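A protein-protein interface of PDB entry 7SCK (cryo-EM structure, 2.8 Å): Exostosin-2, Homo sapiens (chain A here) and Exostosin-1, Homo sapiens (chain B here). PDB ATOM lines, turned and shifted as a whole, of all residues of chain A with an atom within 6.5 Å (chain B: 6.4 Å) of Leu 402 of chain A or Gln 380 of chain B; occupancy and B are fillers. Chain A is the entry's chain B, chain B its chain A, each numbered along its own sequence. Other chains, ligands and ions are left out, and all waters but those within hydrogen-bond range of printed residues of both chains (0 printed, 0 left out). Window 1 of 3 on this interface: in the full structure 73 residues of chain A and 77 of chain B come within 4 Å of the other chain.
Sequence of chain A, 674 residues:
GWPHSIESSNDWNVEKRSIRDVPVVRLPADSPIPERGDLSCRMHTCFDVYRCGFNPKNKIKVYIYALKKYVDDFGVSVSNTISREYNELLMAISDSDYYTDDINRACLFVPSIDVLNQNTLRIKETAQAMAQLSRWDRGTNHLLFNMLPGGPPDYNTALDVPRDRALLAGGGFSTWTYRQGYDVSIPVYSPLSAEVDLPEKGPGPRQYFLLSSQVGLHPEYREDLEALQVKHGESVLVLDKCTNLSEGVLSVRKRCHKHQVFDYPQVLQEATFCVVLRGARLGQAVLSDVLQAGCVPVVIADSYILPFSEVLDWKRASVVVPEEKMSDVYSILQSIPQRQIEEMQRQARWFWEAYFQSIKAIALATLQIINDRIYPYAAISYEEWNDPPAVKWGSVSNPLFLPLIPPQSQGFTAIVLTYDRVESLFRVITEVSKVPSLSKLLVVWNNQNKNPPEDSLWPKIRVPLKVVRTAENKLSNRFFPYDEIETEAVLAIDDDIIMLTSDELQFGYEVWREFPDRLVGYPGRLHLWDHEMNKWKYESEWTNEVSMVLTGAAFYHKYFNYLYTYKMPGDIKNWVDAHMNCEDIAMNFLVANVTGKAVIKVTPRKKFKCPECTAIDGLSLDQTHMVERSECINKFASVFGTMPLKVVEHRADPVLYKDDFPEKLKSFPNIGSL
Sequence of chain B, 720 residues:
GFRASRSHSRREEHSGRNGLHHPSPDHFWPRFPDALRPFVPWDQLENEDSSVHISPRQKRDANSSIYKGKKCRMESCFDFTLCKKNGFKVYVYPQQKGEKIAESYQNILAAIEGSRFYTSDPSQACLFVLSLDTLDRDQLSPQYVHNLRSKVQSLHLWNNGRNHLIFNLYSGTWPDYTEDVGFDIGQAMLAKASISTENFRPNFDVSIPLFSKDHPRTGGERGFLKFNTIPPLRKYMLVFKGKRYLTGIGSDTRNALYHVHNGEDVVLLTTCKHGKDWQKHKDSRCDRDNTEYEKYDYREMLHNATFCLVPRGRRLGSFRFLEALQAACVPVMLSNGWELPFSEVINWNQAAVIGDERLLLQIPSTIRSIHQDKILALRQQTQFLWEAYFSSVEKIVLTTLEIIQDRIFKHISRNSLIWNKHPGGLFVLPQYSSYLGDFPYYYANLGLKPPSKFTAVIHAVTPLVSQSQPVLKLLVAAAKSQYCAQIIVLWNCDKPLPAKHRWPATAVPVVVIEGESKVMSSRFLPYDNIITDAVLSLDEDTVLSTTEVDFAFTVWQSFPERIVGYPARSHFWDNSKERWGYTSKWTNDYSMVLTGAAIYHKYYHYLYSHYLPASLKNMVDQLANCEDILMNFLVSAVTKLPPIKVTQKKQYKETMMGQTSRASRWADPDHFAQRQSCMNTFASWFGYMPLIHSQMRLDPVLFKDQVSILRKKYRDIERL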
ATOM      1  N   ASN A 398     -18.831  -2.517 -10.822  1.00  0.00           N
ATOM      2  CA  ASN A 398     -18.917  -1.636 -11.978  1.00  0.00           C
ATOM      3  C   ASN A 398     -19.205  -0.202 -11.543  1.00  0.00           C
ATOM      4  O   ASN A 398     -20.159   0.030 -10.788  1.00  0.00           O
ATOM      5  CB  ASN A 398     -20.010  -2.134 -12.915  1.00  0.00           C
ATOM      6  CG  ASN A 398     -20.160  -1.275 -14.142  1.00  0.00           C
ATOM      7  OD1 ASN A 398     -19.192  -0.708 -14.643  1.00  0.00           O
ATOM      8  ND2 ASN A 398     -21.382  -1.176 -14.641  1.00  0.00           N
ATOM      9  N   PRO A 399     -18.413   0.781 -11.988  1.00  0.00           N
ATOM     10  CA  PRO A 399     -18.653   2.170 -11.571  1.00  0.00           C
ATOM     11  C   PRO A 399     -19.854   2.810 -12.246  1.00  0.00           C
ATOM     12  O   PRO A 399     -20.579   3.586 -11.618  1.00  0.00           O
ATOM     13  CB  PRO A 399     -17.350   2.875 -11.959  1.00  0.00           C
ATOM     14  CG  PRO A 399     -16.804   2.058 -13.064  1.00  0.00           C
ATOM     15  CD  PRO A 399     -17.156   0.645 -12.740  1.00  0.00           C
ATOM     16  N   LEU A 400     -20.071   2.507 -13.522  1.00  0.00           N
ATOM     17  CA  LEU A 400     -21.200   3.056 -14.267  1.00  0.00           C
ATOM     18  C   LEU A 400     -22.310   2.010 -14.360  1.00  0.00           C
ATOM     19  O   LEU A 400     -22.533   1.383 -15.394  1.00  0.00           O
ATOM     20  CB  LEU A 400     -20.745   3.515 -15.645  1.00  0.00           C
ATOM     21  CG  LEU A 400     -19.485   4.373 -15.647  1.00  0.00           C
ATOM     22  CD1 LEU A 400     -18.977   4.559 -17.062  1.00  0.00           C
ATOM     23  CD2 LEU A 400     -19.760   5.713 -14.993  1.00  0.00           C
ATOM     24  N   PHE A 401     -23.023   1.839 -13.250  1.00  0.00           N
ATOM     25  CA  PHE A 401     -23.980   0.749 -13.129  1.00  0.00           C
ATOM     26  C   PHE A 401     -25.431   1.162 -13.328  1.00  0.00           C
ATOM     27  O   PHE A 401     -26.272   0.288 -13.556  1.00  0.00           O
ATOM     28  CB  PHE A 401     -23.839   0.067 -11.764  1.00  0.00           C
ATOM     29  CG  PHE A 401     -24.009   0.990 -10.591  1.00  0.00           C
ATOM     30  CD1 PHE A 401     -25.264   1.291 -10.103  1.00  0.00           C
ATOM     31  CD2 PHE A 401     -22.910   1.527  -9.954  1.00  0.00           C
ATOM     32  CE1 PHE A 401     -25.419   2.125  -9.019  1.00  0.00           C
ATOM     33  CE2 PHE A 401     -23.058   2.360  -8.868  1.00  0.00           C
ATOM     34  CZ  PHE A 401     -24.315   2.658  -8.399  1.00  0.00           C
ATOM     35  N   LEU A 402     -25.749   2.443 -13.249  1.00  0.00           N
ATOM     36  CA  LEU A 402     -27.147   2.859 -13.272  1.00  0.00           C
ATOM     37  C   LEU A 402     -27.751   2.619 -14.647  1.00  0.00           C
ATOM     38  O   LEU A 402     -27.247   3.160 -15.639  1.00  0.00           O
ATOM     39  CB  LEU A 402     -27.272   4.329 -12.889  1.00  0.00           C
ATOM     40  CG  LEU A 402     -28.700   4.858 -12.773  1.00  0.00           C
ATOM     41  CD1 LEU A 402     -29.460   4.105 -11.701  1.00  0.00           C
ATOM     42  CD2 LEU A 402     -28.694   6.345 -12.482  1.00  0.00           C
ATOM     43  N   PRO A 403     -28.815   1.835 -14.758  1.00  0.00           N
ATOM     44  CA  PRO A 403     -29.415   1.586 -16.073  1.00  0.00           C
ATOM     45  C   PRO A 403     -30.142   2.801 -16.621  1.00  0.00           C
ATOM     46  O   PRO A 403     -31.375   2.857 -16.598  1.00  0.00           O
ATOM     47  CB  PRO A 403     -30.389   0.433 -15.802  1.00  0.00           C
ATOM     48  CG  PRO A 403     -29.941  -0.163 -14.513  1.00  0.00           C
ATOM     49  CD  PRO A 403     -29.404   0.980 -13.720  1.00  0.00           C
ATOM     50  N   LEU A 404     -29.392   3.777 -17.122  1.00  0.00           N
ATOM     51  CA  LEU A 404     -29.962   4.972 -17.718  1.00  0.00           C
ATOM     52  C   LEU A 404     -29.643   4.994 -19.202  1.00  0.00           C
ATOM     53  O   LEU A 404     -28.550   4.597 -19.617  1.00  0.00           O
ATOM     54  CB  LEU A 404     -29.436   6.243 -17.045  1.00  0.00           C
ATOM     55  CG  LEU A 404     -27.935   6.533 -17.108  1.00  0.00           C
ATOM     56  CD1 LEU A 404     -27.589   7.462 -18.266  1.00  0.00           C
ATOM     57  CD2 LEU A 404     -27.452   7.117 -15.794  1.00  0.00           C
ATOM     58  N   ILE A 405     -30.601   5.451 -19.996  1.00  0.00           N
ATOM     59  CA  ILE A 405     -30.439   5.578 -21.437  1.00  0.00           C
ATOM     60  C   ILE A 405     -30.306   7.066 -21.754  1.00  0.00           C
ATOM     61  O   ILE A 405     -31.306   7.797 -21.722  1.00  0.00           O
ATOM     62  CB  ILE A 405     -31.608   4.940 -22.197  1.00  0.00           C
ATOM     63  CG1 ILE A 405     -32.930   5.210 -21.474  1.00  0.00           C
ATOM     64  CG2 ILE A 405     -31.387   3.449 -22.343  1.00  0.00           C
ATOM     65  CD1 ILE A 405     -34.153   4.757 -22.238  1.00  0.00           C
ATOM     66  N   PRO A 516     -24.011   2.160 -22.526  1.00  0.00           N
ATOM     67  CA  PRO A 516     -23.065   3.221 -22.176  1.00  0.00           C
ATOM     68  C   PRO A 516     -22.052   2.845 -21.108  1.00  0.00           C
ATOM     69  O   PRO A 516     -21.409   3.740 -20.552  1.00  0.00           O
ATOM     70  CB  PRO A 516     -23.996   4.331 -21.671  1.00  0.00           C
ATOM     71  CG  PRO A 516     -25.104   3.594 -21.038  1.00  0.00           C
ATOM     72  CD  PRO A 516     -25.302   2.335 -21.839  1.00  0.00           C
ATOM     73  N   LEU B 225     -31.599  12.376 -13.239  1.00  0.00           N
ATOM     74  CA  LEU B 225     -30.276  12.201 -13.827  1.00  0.00           C
ATOM     75  C   LEU B 225     -30.416  11.424 -15.127  1.00  0.00           C
ATOM     76  O   LEU B 225     -30.465  10.193 -15.128  1.00  0.00           O
ATOM     77  CB  LEU B 225     -29.352  11.490 -12.848  1.00  0.00           C
ATOM     78  CG  LEU B 225     -27.850  11.486 -13.114  1.00  0.00           C
ATOM     79  CD1 LEU B 225     -27.094  11.467 -11.802  1.00  0.00           C
ATOM     80  CD2 LEU B 225     -27.451  10.289 -13.953  1.00  0.00           C
ATOM     81  N   ASN B 228     -24.905  11.167 -17.233  1.00  0.00           N
ATOM     82  CA  ASN B 228     -23.882  10.829 -16.248  1.00  0.00           C
ATOM     83  C   ASN B 228     -22.547  11.278 -16.833  1.00  0.00           C
ATOM     84  O   ASN B 228     -21.857  10.510 -17.508  1.00  0.00           O
ATOM     85  CB  ASN B 228     -23.887   9.356 -15.925  1.00  0.00           C
ATOM     86  CG  ASN B 228     -23.141   9.049 -14.653  1.00  0.00           C
ATOM     87  OD1 ASN B 228     -22.422   9.895 -14.129  1.00  0.00           O
ATOM     88  ND2 ASN B 228     -23.306   7.835 -14.146  1.00  0.00           N
ATOM     89  N   ALA B 328     -31.260  13.912  -8.138  1.00  0.00           N
ATOM     90  CA  ALA B 328     -29.950  13.294  -8.317  1.00  0.00           C
ATOM     91  C   ALA B 328     -28.861  13.967  -7.502  1.00  0.00           C
ATOM     92  O   ALA B 328     -27.714  13.512  -7.543  1.00  0.00           O
ATOM     93  CB  ALA B 328     -29.510  13.251  -9.785  1.00  0.00           C
ATOM     94  N   GLN B 350     -23.950   4.813   1.044  1.00  0.00           N
ATOM     95  CA  GLN B 350     -23.711   4.690  -0.383  1.00  0.00           C
ATOM     96  C   GLN B 350     -24.523   5.667  -1.218  1.00  0.00           C
ATOM     97  O   GLN B 350     -24.210   5.847  -2.398  1.00  0.00           O
ATOM     98  CB  GLN B 350     -24.023   3.267  -0.853  1.00  0.00           C
ATOM     99  CG  GLN B 350     -23.193   2.183  -0.198  1.00  0.00           C
ATOM    100  CD  GLN B 350     -23.529   0.804  -0.727  1.00  0.00           C
ATOM    101  OE1 GLN B 350     -24.278   0.663  -1.693  1.00  0.00           O
ATOM    102  NE2 GLN B 350     -22.976  -0.225  -0.094  1.00  0.00           N
ATOM    103  N   ILE B 375     -18.483  10.606  -5.472  1.00  0.00           N
ATOM    104  CA  ILE B 375     -19.642  11.388  -5.897  1.00  0.00           C
ATOM    105  C   ILE B 375     -20.401  10.666  -7.001  1.00  0.00           C
ATOM    106  O   ILE B 375     -21.639  10.645  -7.012  1.00  0.00           O
ATOM    107  CB  ILE B 375     -19.206  12.798  -6.334  1.00  0.00           C
ATOM    108  CG1 ILE B 375     -18.685  13.583  -5.135  1.00  0.00           C
ATOM    109  CG2 ILE B 375     -20.356  13.538  -6.973  1.00  0.00           C
ATOM    110  CD1 ILE B 375     -18.166  14.954  -5.480  1.00  0.00           C
ATOM    111  N   LEU B 376     -19.677  10.074  -7.951  1.00  0.00           N
ATOM    112  CA  LEU B 376     -20.332   9.325  -9.018  1.00  0.00           C
ATOM    113  C   LEU B 376     -21.154   8.178  -8.445  1.00  0.00           C
ATOM    114  O   LEU B 376     -22.333   7.991  -8.793  1.00  0.00           O
ATOM    115  CB  LEU B 376     -19.281   8.803  -9.997  1.00  0.00           C
ATOM    116  CG  LEU B 376     -19.736   8.597 -11.436  1.00  0.00           C
ATOM    117  CD1 LEU B 376     -20.010   9.940 -12.087  1.00  0.00           C
ATOM    118  CD2 LEU B 376     -18.692   7.825 -12.214  1.00  0.00           C
ATOM    119  N   ALA B 377     -20.553   7.421  -7.523  1.00  0.00           N
ATOM    120  CA  ALA B 377     -21.261   6.316  -6.892  1.00  0.00           C
ATOM    121  C   ALA B 377     -22.476   6.807  -6.119  1.00  0.00           C
ATOM    122  O   ALA B 377     -23.546   6.194  -6.184  1.00  0.00           O
ATOM    123  CB  ALA B 377     -20.316   5.549  -5.971  1.00  0.00           C
ATOM    124  N   LEU B 378     -22.332   7.910  -5.380  1.00  0.00           N
ATOM    125  CA  LEU B 378     -23.436   8.419  -4.574  1.00  0.00           C
ATOM    126  C   LEU B 378     -24.605   8.857  -5.443  1.00  0.00           C
ATOM    127  O   LEU B 378     -25.765   8.569  -5.124  1.00  0.00           O
ATOM    128  CB  LEU B 378     -22.957   9.573  -3.703  1.00  0.00           C
ATOM    129  CG  LEU B 378     -22.055   9.245  -2.517  1.00  0.00           C
ATOM    130  CD1 LEU B 378     -21.362  10.501  -2.030  1.00  0.00           C
ATOM    131  CD2 LEU B 378     -22.850   8.620  -1.395  1.00  0.00           C
ATOM    132  N   ARG B 379     -24.323   9.557  -6.542  1.00  0.00           N
ATOM    133  CA  ARG B 379     -25.394   9.988  -7.432  1.00  0.00           C
ATOM    134  C   ARG B 379     -26.121   8.793  -8.031  1.00  0.00           C
ATOM    135  O   ARG B 379     -27.361   8.737  -8.041  1.00  0.00           O
ATOM    136  CB  ARG B 379     -24.833  10.879  -8.538  1.00  0.00           C
ATOM    137  CG  ARG B 379     -24.396  12.249  -8.078  1.00  0.00           C
ATOM    138  CD  ARG B 379     -23.816  13.054  -9.225  1.00  0.00           C
ATOM    139  NE  ARG B 379     -24.047  12.419 -10.517  1.00  0.00           N
ATOM    140  CZ  ARG B 379     -23.638  12.912 -11.677  1.00  0.00           C
ATOM    141  NH1 ARG B 379     -22.986  14.058 -11.749  1.00  0.00           N
ATOM    142  NH2 ARG B 379     -23.892  12.237 -12.794  1.00  0.00           N
ATOM    143  N   GLN B 380     -25.365   7.813  -8.528  1.00  0.00           N
ATOM    144  CA  GLN B 380     -26.020   6.653  -9.117  1.00  0.00           C
ATOM    145  C   GLN B 380     -26.829   5.889  -8.074  1.00  0.00           C
ATOM    146  O   GLN B 380     -27.934   5.413  -8.361  1.00  0.00           O
ATOM    147  CB  GLN B 380     -24.986   5.757  -9.789  1.00  0.00           C
ATOM    148  CG  GLN B 380     -24.251   6.449 -10.922  1.00  0.00           C
ATOM    149  CD  GLN B 380     -23.359   5.515 -11.699  1.00  0.00           C
ATOM    150  OE1 GLN B 380     -23.474   4.295 -11.588  1.00  0.00           O
ATOM    151  NE2 GLN B 380     -22.457   6.080 -12.487  1.00  0.00           N
ATOM    152  N   GLN B 381     -26.313   5.791  -6.849  1.00  0.00           N
ATOM    153  CA  GLN B 381     -27.009   5.040  -5.813  1.00  0.00           C
ATOM    154  C   GLN B 381     -28.287   5.741  -5.378  1.00  0.00           C
ATOM    155  O   GLN B 381     -29.305   5.082  -5.135  1.00  0.00           O
ATOM    156  CB  GLN B 381     -26.085   4.818  -4.620  1.00  0.00           C
ATOM    157  CG  GLN B 381     -26.618   3.860  -3.576  1.00  0.00           C
ATOM    158  CD  GLN B 381     -26.611   2.420  -4.033  1.00  0.00           C
ATOM    159  OE1 GLN B 381     -26.135   2.100  -5.119  1.00  0.00           O
ATOM    160  NE2 GLN B 381     -27.139   1.537  -3.199  1.00  0.00           N
ATOM    161  N   THR B 382     -28.264   7.072  -5.269  1.00  0.00           N
ATOM    162  CA  THR B 382     -29.481   7.774  -4.875  1.00  0.00           C
ATOM    163  C   THR B 382     -30.531   7.687  -5.975  1.00  0.00           C
ATOM    164  O   THR B 382     -31.729   7.546  -5.695  1.00  0.00           O
ATOM    165  CB  THR B 382     -29.180   9.232  -4.500  1.00  0.00           C
ATOM    166  OG1 THR B 382     -30.381   9.860  -4.040  1.00  0.00           O
ATOM    167  CG2 THR B 382     -28.661  10.021  -5.668  1.00  0.00           C
ATOM    168  N   GLN B 383     -30.101   7.721  -7.239  1.00  0.00           N
ATOM    169  CA  GLN B 383     -31.056   7.520  -8.322  1.00  0.00           C
ATOM    170  C   GLN B 383     -31.663   6.123  -8.277  1.00  0.00           C
ATOM    171  O   GLN B 383     -32.874   5.955  -8.481  1.00  0.00           O
ATOM    172  CB  GLN B 383     -30.388   7.772  -9.668  1.00  0.00           C
ATOM    173  CG  GLN B 383     -30.285   9.229 -10.019  1.00  0.00           C
ATOM    174  CD  GLN B 383     -31.633   9.893 -10.082  1.00  0.00           C
ATOM    175  OE1 GLN B 383     -32.393   9.686 -11.024  1.00  0.00           O
ATOM    176  NE2 GLN B 383     -31.945  10.691  -9.073  1.00  0.00           N
ATOM    177  N   PHE B 384     -30.839   5.108  -8.008  1.00  0.00           N
ATOM    178  CA  PHE B 384     -31.358   3.747  -7.902  1.00  0.00           C
ATOM    179  C   PHE B 384     -32.355   3.623  -6.758  1.00  0.00           C
ATOM    180  O   PHE B 384     -33.418   3.009  -6.910  1.00  0.00           O
ATOM    181  CB  PHE B 384     -30.212   2.756  -7.714  1.00  0.00           C
ATOM    182  CG  PHE B 384     -30.637   1.458  -7.095  1.00  0.00           C
ATOM    183  CD1 PHE B 384     -31.332   0.521  -7.829  1.00  0.00           C
ATOM    184  CD2 PHE B 384     -30.351   1.184  -5.777  1.00  0.00           C
ATOM    185  CE1 PHE B 384     -31.727  -0.663  -7.257  1.00  0.00           C
ATOM    186  CE2 PHE B 384     -30.740   0.001  -5.205  1.00  0.00           C
ATOM    187  CZ  PHE B 384     -31.432  -0.920  -5.943  1.00  0.00           C
ATOM    188  N   LEU B 385     -32.023   4.193  -5.600  1.00  0.00           N
ATOM    189  CA  LEU B 385     -32.920   4.112  -4.453  1.00  0.00           C
ATOM    190  C   LEU B 385     -34.248   4.788  -4.747  1.00  0.00           C
ATOM    191  O   LEU B 385     -35.312   4.255  -4.408  1.00  0.00           O
ATOM    192  CB  LEU B 385     -32.272   4.736  -3.227  1.00  0.00           C
ATOM    193  CG  LEU B 385     -31.159   3.934  -2.579  1.00  0.00           C
ATOM    194  CD1 LEU B 385     -30.765   4.590  -1.284  1.00  0.00           C
ATOM    195  CD2 LEU B 385     -31.614   2.516  -2.336  1.00  0.00           C
ATOM    196  N   GLU B 387     -35.657   5.224  -7.767  1.00  0.00           N
ATOM    197  CA  GLU B 387     -36.426   4.479  -8.754  1.00  0.00           C
ATOM    198  C   GLU B 387     -36.909   3.136  -8.229  1.00  0.00           C
ATOM    199  O   GLU B 387     -37.837   2.561  -8.803  1.00  0.00           O
ATOM    200  CB  GLU B 387     -35.602   4.274 -10.023  1.00  0.00           C
ATOM    201  CG  GLU B 387     -35.272   5.557 -10.763  1.00  0.00           C
ATOM    202  CD  GLU B 387     -34.481   5.314 -12.033  1.00  0.00           C
ATOM    203  OE1 GLU B 387     -34.178   4.140 -12.332  1.00  0.00           O
ATOM    204  OE2 GLU B 387     -34.162   6.297 -12.734  1.00  0.00           O
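The side-chain amide oxygen (OE1) of Gln 380 of chain B sits at hydrogen-bond distance from the backbone NH (N) of Leu 402 of chain A, 3.4 Å away. The side-chain amide oxygen (OE1) of Gln 380 of chain B sits close to the backbone carbonyl oxygen (O) of Pro 399 of chain A (3.0 Å). The side-chain amide oxygen of Gln 380 of chain B is in hydrogen-bond range of the backbone NH of Phe 401 of chain A (3.0 Å).
NE2 of Gln 381 of chain B is in hydrogen-bond range of OE1 of Gln 350 of chain B (3.3 Å). The backbone carbonyl oxygen (O) of Leu 400 of chain A sits at hydrogen-bond distance from the side-chain amide nitrogen (ND2) of Asn 398 of chain A (2.9 Å). The side-chain amide nitrogen of Gln 383 of chain B lies close to the backbone NH of Ala 328 of chain B. The side-chain amide nitrogen (NE2) of Gln 380 of chain B sits close to the side-chain amide nitrogen (ND2) of Asn 228 of chain B, 2.6 Å away.
Leu 400 of chain A touches Leu 376 of chain B (CD2 to CD2, 3.7 Å). Gln 380 of chain B touches Leu 400 of chain A (NE2 to CD2, 3.7 Å). OE1 of Gln 381 of chain B touches CZ of Phe 401 of chain A, 3.8 Å away. Leu 402 of chain A touches Gln 383 of chain B. Leu 404 of chain A touches Leu 225 of chain B.
Of the printed residues of chain B, Phe 401 of chain A touches Gln 380 and Gln 381. Of chain B, only Gln 380 and Gln 383 come within 4 Å of Leu 402 of chain A. Of the printed residues of chain B, Leu 404 of chain A touches Leu 225. Ala 328 of chain B touches none of the printed residues of chain A. Printed residues of chain A within 4 Å of Gln 380 of chain B: Pro 399, Leu 400, Phe 401 and Leu 402. Glu 387 of chain B touches none of the printed residues of chain A. The nearest printed residue of chain A that does not touch Leu 376 of chain B is Pro 399 of chain A (4.7 Å).
Printed residues of chain B that touch a printed residue of chain A: Leu 225, Leu 376, Gln 380, Gln 381 and Gln 383.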
